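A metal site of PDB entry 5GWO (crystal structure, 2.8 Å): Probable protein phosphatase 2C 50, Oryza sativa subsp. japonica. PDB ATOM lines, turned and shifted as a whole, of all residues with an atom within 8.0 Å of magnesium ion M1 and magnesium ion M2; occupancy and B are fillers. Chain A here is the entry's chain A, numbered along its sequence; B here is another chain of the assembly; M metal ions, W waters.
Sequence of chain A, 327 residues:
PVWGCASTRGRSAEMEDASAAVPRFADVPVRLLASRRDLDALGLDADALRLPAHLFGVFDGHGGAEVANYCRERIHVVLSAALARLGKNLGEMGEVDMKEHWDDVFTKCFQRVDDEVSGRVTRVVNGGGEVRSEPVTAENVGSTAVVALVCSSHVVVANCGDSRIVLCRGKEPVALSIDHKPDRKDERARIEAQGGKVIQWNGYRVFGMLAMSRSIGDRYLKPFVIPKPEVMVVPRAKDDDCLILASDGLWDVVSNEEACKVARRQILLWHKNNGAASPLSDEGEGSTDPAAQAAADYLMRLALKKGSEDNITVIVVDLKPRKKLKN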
ATOM      1  N   SER A  12      31.686 -12.904  19.052  1.00  0.00           N
ATOM      2  CA  SER A  12      31.853 -11.815  19.987  1.00  0.00           C
ATOM      3  C   SER A  12      33.243 -11.868  20.608  1.00  0.00           C
ATOM      4  O   SER A  12      33.898 -12.910  20.637  1.00  0.00           O
ATOM      5  CB  SER A  12      30.782 -11.861  21.062  1.00  0.00           C
ATOM      6  OG  SER A  12      29.500 -11.755  20.463  1.00  0.00           O
ATOM      7  N   GLU A  14      34.193 -11.026  23.914  1.00  0.00           N
ATOM      8  CA  GLU A  14      34.168 -11.608  25.241  1.00  0.00           C
ATOM      9  C   GLU A  14      33.011 -12.597  25.354  1.00  0.00           C
ATOM     10  O   GLU A  14      32.030 -12.533  24.620  1.00  0.00           O
ATOM     11  CB  GLU A  14      34.022 -10.533  26.316  1.00  0.00           C
ATOM     12  CG  GLU A  14      35.036  -9.408  26.243  1.00  0.00           C
ATOM     13  CD  GLU A  14      34.682  -8.236  27.147  1.00  0.00           C
ATOM     14  OE1 GLU A  14      33.493  -7.842  27.163  1.00  0.00           O
ATOM     15  OE2 GLU A  14      35.577  -7.691  27.813  1.00  0.00           O
ATOM     16  N   MET A  15      33.154 -13.518  26.304  1.00  0.00           N
ATOM     17  CA  MET A  15      32.107 -14.486  26.605  1.00  0.00           C
ATOM     18  C   MET A  15      31.310 -13.966  27.798  1.00  0.00           C
ATOM     19  O   MET A  15      31.869 -13.732  28.875  1.00  0.00           O
ATOM     20  CB  MET A  15      32.687 -15.869  26.923  1.00  0.00           C
ATOM     21  CG  MET A  15      31.629 -16.891  27.279  1.00  0.00           C
ATOM     22  SD  MET A  15      30.315 -16.985  26.035  1.00  0.00           S
ATOM     23  CE  MET A  15      29.833 -18.698  26.164  1.00  0.00           C
ATOM     24  N   GLU A  16      30.026 -13.725  27.587  1.00  0.00           N
ATOM     25  CA  GLU A  16      29.141 -13.272  28.648  1.00  0.00           C
ATOM     26  C   GLU A  16      27.944 -14.199  28.843  1.00  0.00           C
ATOM     27  O   GLU A  16      27.003 -13.857  29.552  1.00  0.00           O
ATOM     28  CB  GLU A  16      28.696 -11.830  28.382  1.00  0.00           C
ATOM     29  CG  GLU A  16      29.868 -10.847  28.426  1.00  0.00           C
ATOM     30  CD  GLU A  16      29.467  -9.424  28.125  1.00  0.00           C
ATOM     31  OE1 GLU A  16      28.304  -9.211  27.723  1.00  0.00           O
ATOM     32  OE2 GLU A  16      30.314  -8.510  28.278  1.00  0.00           O
ATOM     33  N   ASP A  17      27.935 -15.347  28.186  1.00  0.00           N
ATOM     34  CA  ASP A  17      26.927 -16.356  28.468  1.00  0.00           C
ATOM     35  C   ASP A  17      27.452 -17.325  29.521  1.00  0.00           C
ATOM     36  O   ASP A  17      28.656 -17.464  29.733  1.00  0.00           O
ATOM     37  CB  ASP A  17      26.518 -17.099  27.190  1.00  0.00           C
ATOM     38  CG  ASP A  17      25.553 -16.283  26.313  1.00  0.00           C
ATOM     39  OD1 ASP A  17      25.558 -15.035  26.412  1.00  0.00           O
ATOM     40  OD2 ASP A  17      24.811 -16.900  25.517  1.00  0.00           O
ATOM     41  N   PHE A  59      22.030 -18.579  30.933  1.00  0.00           N
ATOM     42  CA  PHE A  59      22.111 -17.214  31.458  1.00  0.00           C
ATOM     43  C   PHE A  59      22.874 -16.382  30.430  1.00  0.00           C
ATOM     44  O   PHE A  59      24.103 -16.422  30.360  1.00  0.00           O
ATOM     45  CB  PHE A  59      22.763 -17.191  32.840  1.00  0.00           C
ATOM     46  CG  PHE A  59      22.292 -18.285  33.761  1.00  0.00           C
ATOM     47  CD1 PHE A  59      21.072 -18.198  34.395  1.00  0.00           C
ATOM     48  CD2 PHE A  59      23.071 -19.405  33.981  1.00  0.00           C
ATOM     49  CE1 PHE A  59      20.621 -19.214  35.221  1.00  0.00           C
ATOM     50  CE2 PHE A  59      22.639 -20.426  34.819  1.00  0.00           C
ATOM     51  CZ  PHE A  59      21.403 -20.323  35.433  1.00  0.00           C
ATOM     52  N   ASP A  60      22.136 -15.637  29.619  1.00  0.00           N
ATOM     53  CA  ASP A  60      22.723 -14.719  28.660  1.00  0.00           C
ATOM     54  C   ASP A  60      23.025 -13.416  29.395  1.00  0.00           C
ATOM     55  O   ASP A  60      22.103 -12.665  29.742  1.00  0.00           O
ATOM     56  CB  ASP A  60      21.799 -14.495  27.469  1.00  0.00           C
ATOM     57  CG  ASP A  60      22.370 -13.530  26.445  1.00  0.00           C
ATOM     58  OD1 ASP A  60      23.503 -13.024  26.643  1.00  0.00           O
ATOM     59  OD2 ASP A  60      21.688 -13.290  25.421  1.00  0.00           O
ATOM     60  N   GLY A  61      24.295 -13.183  29.683  1.00  0.00           N
ATOM     61  CA  GLY A  61      24.674 -11.952  30.323  1.00  0.00           C
ATOM     62  C   GLY A  61      24.766 -10.798  29.342  1.00  0.00           C
ATOM     63  O   GLY A  61      24.844 -10.980  28.117  1.00  0.00           O
ATOM     64  N   HIS A  62      24.729  -9.601  29.903  1.00  0.00           N
ATOM     65  CA  HIS A  62      24.925  -8.387  29.124  1.00  0.00           C
ATOM     66  C   HIS A  62      25.509  -7.316  30.032  1.00  0.00           C
ATOM     67  O   HIS A  62      25.314  -7.333  31.251  1.00  0.00           O
ATOM     68  CB  HIS A  62      23.609  -7.949  28.478  1.00  0.00           C
ATOM     69  CG  HIS A  62      22.497  -7.758  29.447  1.00  0.00           C
ATOM     70  ND1 HIS A  62      21.337  -8.499  29.396  1.00  0.00           N
ATOM     71  CD2 HIS A  62      22.370  -6.926  30.502  1.00  0.00           C
ATOM     72  CE1 HIS A  62      20.534  -8.127  30.375  1.00  0.00           C
ATOM     73  NE2 HIS A  62      21.142  -7.175  31.069  1.00  0.00           N
ATOM     74  N   GLY A  63      26.257  -6.392  29.425  1.00  0.00           N
ATOM     75  CA  GLY A  63      26.956  -5.392  30.202  1.00  0.00           C
ATOM     76  C   GLY A  63      28.062  -5.951  31.062  1.00  0.00           C
ATOM     77  O   GLY A  63      28.598  -5.226  31.910  1.00  0.00           O
ATOM     78  N   GLY A  64      28.434  -7.208  30.850  1.00  0.00           N
ATOM     79  CA  GLY A  64      29.329  -7.940  31.720  1.00  0.00           C
ATOM     80  C   GLY A  64      28.831  -9.366  31.915  1.00  0.00           C
ATOM     81  O   GLY A  64      27.678  -9.681  31.654  1.00  0.00           O
ATOM     82  N   ALA A  68      25.500 -13.309  34.958  1.00  0.00           N
ATOM     83  CA  ALA A  68      25.217 -14.657  34.459  1.00  0.00           C
ATOM     84  C   ALA A  68      26.005 -15.700  35.248  1.00  0.00           C
ATOM     85  O   ALA A  68      25.475 -16.771  35.560  1.00  0.00           O
ATOM     86  CB  ALA A  68      25.525 -14.744  32.967  1.00  0.00           C
ATOM     87  N   GLY A 142      23.524  -7.200  33.789  1.00  0.00           N
ATOM     88  CA  GLY A 142      22.361  -8.024  34.038  1.00  0.00           C
ATOM     89  C   GLY A 142      22.531  -9.371  33.368  1.00  0.00           C
ATOM     90  O   GLY A 142      23.627  -9.699  32.911  1.00  0.00           O
ATOM     91  N   SER A 143      21.468 -10.168  33.311  1.00  0.00           N
ATOM     92  CA  SER A 143      21.574 -11.470  32.679  1.00  0.00           C
ATOM     93  C   SER A 143      20.184 -12.048  32.478  1.00  0.00           C
ATOM     94  O   SER A 143      19.315 -11.862  33.342  1.00  0.00           O
ATOM     95  CB  SER A 143      22.422 -12.434  33.511  1.00  0.00           C
ATOM     96  OG  SER A 143      22.379 -13.726  32.940  1.00  0.00           O
ATOM     97  N   THR A 144      19.962 -12.697  31.344  1.00  0.00           N
ATOM     98  CA  THR A 144      18.769 -13.520  31.267  1.00  0.00           C
ATOM     99  C   THR A 144      18.967 -14.748  32.137  1.00  0.00           C
ATOM    100  O   THR A 144      20.087 -15.056  32.566  1.00  0.00           O
ATOM    101  CB  THR A 144      18.430 -13.934  29.816  1.00  0.00           C
ATOM    102  OG1 THR A 144      19.347 -14.925  29.324  1.00  0.00           O
ATOM    103  CG2 THR A 144      18.438 -12.741  28.883  1.00  0.00           C
ATOM    104  N   ASP A 162      15.218 -13.060  27.279  1.00  0.00           N
ATOM    105  CA  ASP A 162      15.030 -13.441  25.887  1.00  0.00           C
ATOM    106  C   ASP A 162      15.648 -14.785  25.544  1.00  0.00           C
ATOM    107  O   ASP A 162      15.693 -15.162  24.371  1.00  0.00           O
ATOM    108  CB  ASP A 162      15.563 -12.350  24.935  1.00  0.00           C
ATOM    109  CG  ASP A 162      17.071 -12.145  25.048  1.00  0.00           C
ATOM    110  OD1 ASP A 162      17.784 -13.033  25.548  1.00  0.00           O
ATOM    111  OD2 ASP A 162      17.540 -11.081  24.597  1.00  0.00           O
ATOM    112  N   SER A 163      16.166 -15.497  26.541  1.00  0.00           N
ATOM    113  CA  SER A 163      16.512 -16.887  26.311  1.00  0.00           C
ATOM    114  C   SER A 163      15.243 -17.731  26.241  1.00  0.00           C
ATOM    115  O   SER A 163      14.153 -17.308  26.634  1.00  0.00           O
ATOM    116  CB  SER A 163      17.452 -17.397  27.399  1.00  0.00           C
ATOM    117  OG  SER A 163      18.652 -16.635  27.420  1.00  0.00           O
ATOM    118  N   MET A 212      14.965  -6.228  26.318  1.00  0.00           N
ATOM    119  CA  MET A 212      14.190  -7.200  27.068  1.00  0.00           C
ATOM    120  C   MET A 212      13.571  -6.475  28.249  1.00  0.00           C
ATOM    121  O   MET A 212      14.093  -5.465  28.725  1.00  0.00           O
ATOM    122  CB  MET A 212      15.031  -8.396  27.512  1.00  0.00           C
ATOM    123  CG  MET A 212      16.207  -8.010  28.362  1.00  0.00           C
ATOM    124  SD  MET A 212      17.165  -9.443  28.877  1.00  0.00           S
ATOM    125  CE  MET A 212      17.674 -10.076  27.286  1.00  0.00           C
ATOM    126  N   SER A 247      20.492 -19.466  24.540  1.00  0.00           N
ATOM    127  CA  SER A 247      20.471 -18.008  24.489  1.00  0.00           C
ATOM    128  C   SER A 247      19.915 -17.515  23.157  1.00  0.00           C
ATOM    129  O   SER A 247      19.641 -18.292  22.232  1.00  0.00           O
ATOM    130  CB  SER A 247      21.886 -17.475  24.723  1.00  0.00           C
ATOM    131  OG  SER A 247      22.834 -18.230  23.991  1.00  0.00           O
ATOM    132  N   ASP A 248      19.719 -16.190  23.050  1.00  0.00           N
ATOM    133  CA  ASP A 248      19.244 -15.622  21.786  1.00  0.00           C
ATOM    134  C   ASP A 248      20.200 -15.931  20.641  1.00  0.00           C
ATOM    135  O   ASP A 248      19.774 -15.972  19.481  1.00  0.00           O
ATOM    136  CB  ASP A 248      18.995 -14.103  21.886  1.00  0.00           C
ATOM    137  CG  ASP A 248      20.181 -13.331  22.448  1.00  0.00           C
ATOM    138  OD1 ASP A 248      21.277 -13.885  22.621  1.00  0.00           O
ATOM    139  OD2 ASP A 248      20.016 -12.119  22.707  1.00  0.00           O
ATOM    140  N   GLY A 249      21.475 -16.205  20.949  1.00  0.00           N
ATOM    141  CA  GLY A 249      22.460 -16.546  19.951  1.00  0.00           C
ATOM    142  C   GLY A 249      22.086 -17.746  19.101  1.00  0.00           C
ATOM    143  O   GLY A 249      22.716 -17.969  18.057  1.00  0.00           O
ATOM    144  N   LEU A 250      21.080 -18.514  19.514  1.00  0.00           N
ATOM    145  CA  LEU A 250      20.576 -19.615  18.716  1.00  0.00           C
ATOM    146  C   LEU A 250      19.209 -19.326  18.129  1.00  0.00           C
ATOM    147  O   LEU A 250      18.981 -19.592  16.939  1.00  0.00           O
ATOM    148  CB  LEU A 250      20.529 -20.891  19.559  1.00  0.00           C
ATOM    149  CG  LEU A 250      19.803 -22.094  18.934  1.00  0.00           C
ATOM    150  CD1 LEU A 250      20.461 -22.518  17.616  1.00  0.00           C
ATOM    151  CD2 LEU A 250      19.799 -23.244  19.915  1.00  0.00           C
ATOM    152  N   ASP A 252      17.868 -16.495  17.419  1.00  0.00           N
ATOM    153  CA  ASP A 252      17.832 -15.388  16.477  1.00  0.00           C
ATOM    154  C   ASP A 252      18.068 -15.848  15.039  1.00  0.00           C
ATOM    155  O   ASP A 252      17.610 -15.171  14.112  1.00  0.00           O
ATOM    156  CB  ASP A 252      18.861 -14.330  16.864  1.00  0.00           C
ATOM    157  CG  ASP A 252      18.429 -13.490  18.057  1.00  0.00           C
ATOM    158  OD1 ASP A 252      17.216 -13.527  18.380  1.00  0.00           O
ATOM    159  OD2 ASP A 252      19.277 -12.813  18.667  1.00  0.00           O
ATOM    160  N   SER A 308      25.507 -16.262  13.385  1.00  0.00           N
ATOM    161  CA  SER A 308      25.148 -15.692  14.687  1.00  0.00           C
ATOM    162  C   SER A 308      26.358 -14.976  15.255  1.00  0.00           C
ATOM    163  O   SER A 308      27.426 -15.570  15.414  1.00  0.00           O
ATOM    164  CB  SER A 308      24.660 -16.780  15.646  1.00  0.00           C
ATOM    165  OG  SER A 308      24.250 -16.225  16.886  1.00  0.00           O
ATOM    166  N   GLU A 309      26.198 -13.691  15.567  1.00  0.00           N
ATOM    167  CA  GLU A 309      27.311 -12.909  16.070  1.00  0.00           C
ATOM    168  C   GLU A 309      27.301 -12.749  17.593  1.00  0.00           C
ATOM    169  O   GLU A 309      28.162 -12.058  18.128  1.00  0.00           O
ATOM    170  CB  GLU A 309      27.332 -11.535  15.398  1.00  0.00           C
ATOM    171  CG  GLU A 309      27.709 -11.613  13.930  1.00  0.00           C
ATOM    172  CD  GLU A 309      27.347 -10.368  13.172  1.00  0.00           C
ATOM    173  OE1 GLU A 309      26.291  -9.779  13.472  1.00  0.00           O
ATOM    174  OE2 GLU A 309      28.107  -9.982  12.254  1.00  0.00           O
ATOM    175  N   ASP A 310      26.374 -13.400  18.287  1.00  0.00           N
ATOM    176  CA  ASP A 310      26.302 -13.331  19.740  1.00  0.00           C
ATOM    177  C   ASP A 310      26.969 -14.564  20.351  1.00  0.00           C
ATOM    178  O   ASP A 310      27.291 -15.536  19.658  1.00  0.00           O
ATOM    179  CB  ASP A 310      24.846 -13.207  20.197  1.00  0.00           C
ATOM    180  CG  ASP A 310      24.708 -12.834  21.673  1.00  0.00           C
ATOM    181  OD1 ASP A 310      25.686 -12.329  22.277  1.00  0.00           O
ATOM    182  OD2 ASP A 310      23.622 -13.053  22.243  1.00  0.00           O
ATOM    183  N   ASN A 311      27.213 -14.489  21.663  1.00  0.00           N
ATOM    184  CA  ASN A 311      27.585 -15.680  22.402  1.00  0.00           C
ATOM    185  C   ASN A 311      26.496 -16.734  22.219  1.00  0.00           C
ATOM    186  O   ASN A 311      25.302 -16.414  22.255  1.00  0.00           O
ATOM    187  CB  ASN A 311      27.747 -15.378  23.896  1.00  0.00           C
ATOM    188  CG  ASN A 311      28.703 -14.236  24.176  1.00  0.00           C
ATOM    189  OD1 ASN A 311      28.574 -13.551  25.204  1.00  0.00           O
ATOM    190  ND2 ASN A 311      29.668 -14.011  23.282  1.00  0.00           N
ATOM    191  N   ILE A 312      26.905 -17.980  22.021  1.00  0.00           N
ATOM    192  CA  ILE A 312      25.964 -19.066  21.785  1.00  0.00           C
ATOM    193  C   ILE A 312      26.068 -20.080  22.912  1.00  0.00           C
ATOM    194  O   ILE A 312      27.151 -20.585  23.207  1.00  0.00           O
ATOM    195  CB  ILE A 312      26.209 -19.751  20.422  1.00  0.00           C
ATOM    196  CG1 ILE A 312      26.025 -18.738  19.301  1.00  0.00           C
ATOM    197  CG2 ILE A 312      25.267 -20.940  20.264  1.00  0.00           C
ATOM    198  CD1 ILE A 312      26.403 -19.282  17.944  1.00  0.00           C
ATOM    199  N   SER B  71      27.624  -4.695  26.072  1.00  0.00           N
ATOM    200  CA  SER B  71      26.386  -5.252  25.551  1.00  0.00           C
ATOM    201  C   SER B  71      25.210  -4.695  26.325  1.00  0.00           C
ATOM    202  O   SER B  71      25.346  -4.009  27.336  1.00  0.00           O
ATOM    203  CB  SER B  71      26.429  -6.777  25.616  1.00  0.00           C
ATOM    204  OG  SER B  71      26.935  -7.200  26.867  1.00  0.00           O
ATOM    205  N   GLY B  72      24.011  -4.961  25.811  1.00  0.00           N
ATOM    206  CA  GLY B  72      22.791  -4.428  26.393  1.00  0.00           C
ATOM    207  C   GLY B  72      22.403  -3.065  25.870  1.00  0.00           C
ATOM    208  O   GLY B  72      21.656  -2.347  26.549  1.00  0.00           O
HETATM  209 MG    MG M   1      22.834 -12.436  23.716  1.00  0.00          MG
HETATM  210 MG    MG M   2      24.436 -11.176  26.014  1.00  0.00          MG
HETATM  211 MG    MG M   3      17.853 -11.467  21.030  1.00  0.00          MG
HETATM  212  O   HOH W   1      23.189 -14.694  23.709  1.00  0.00           O
HETATM  213  O   HOH W   2      22.822  -9.119  25.197  1.00  0.00           O
HETATM  214  O   HOH W   3      26.195 -10.209  25.254  1.00  0.00           O
HETATM  215  O   HOH W   4      20.050 -10.688  24.652  1.00  0.00           O
HETATM  216  O   HOH W   5      26.087 -12.436  26.344  1.00  0.00           O
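The nearest printed residue that does not touch magnesium ion M2 is Asp 17 (4.04 Å).
Magnesium ion M2 is bound by water W5 (2.1 Å), water W3 (2.1 Å), O of Gly 61 (2.2 Å) and OD1 of Asp 60 (2.2 Å). Slightly farther from magnesium ion M2 lies water W2 (2.7 Å).
Magnesium ion M1 is bound by the side-chain carboxylate of Asp 310 (1.8 Å), the side-chain carboxylate of Asp 60 (2.2 Å), water W1 (2.3 Å) and the side-chain carboxylate of Asp 248 (2.4 Å). Magnesium ion M1 has four donor atoms within binding distance.
Of the 30 residues printed, 3 come within 4 Å of magnesium ion M1.
The backbone carbonyl oxygen of Glu 16 sits at hydrogen-bond distance from the backbone NH of Gly 61, at 2.8 Å. The backbone carbonyl oxygen (O) of Asp 60 sits at hydrogen-bond distance from the backbone NH (N) of Thr 144 (2.7 Å). The backbone carbonyl oxygen (O) of Asp 60 lies close to the side-chain hydroxyl (OG) of Ser 143 (3.4 Å).
Water W1 lies within hydrogen-bond range of O of Asn 311 (3.1 Å) and OD2 of Asp 17 (3.3 Å). Water W3 bridges the side-chain carboxylate of Glu 16 (3.4 Å) and the side-chain hydroxyl of Ser 71 of chain B (3.5 Å). Water W5 lies within hydrogen-bond range of OD1 of Asp 17 (2.7 Å) and OD1 of Asn 311 (3.0 Å). Water W4 bridges OD2 of Asp 248 (2.4 Å) and OD2 of Asp 162 (2.5 Å).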
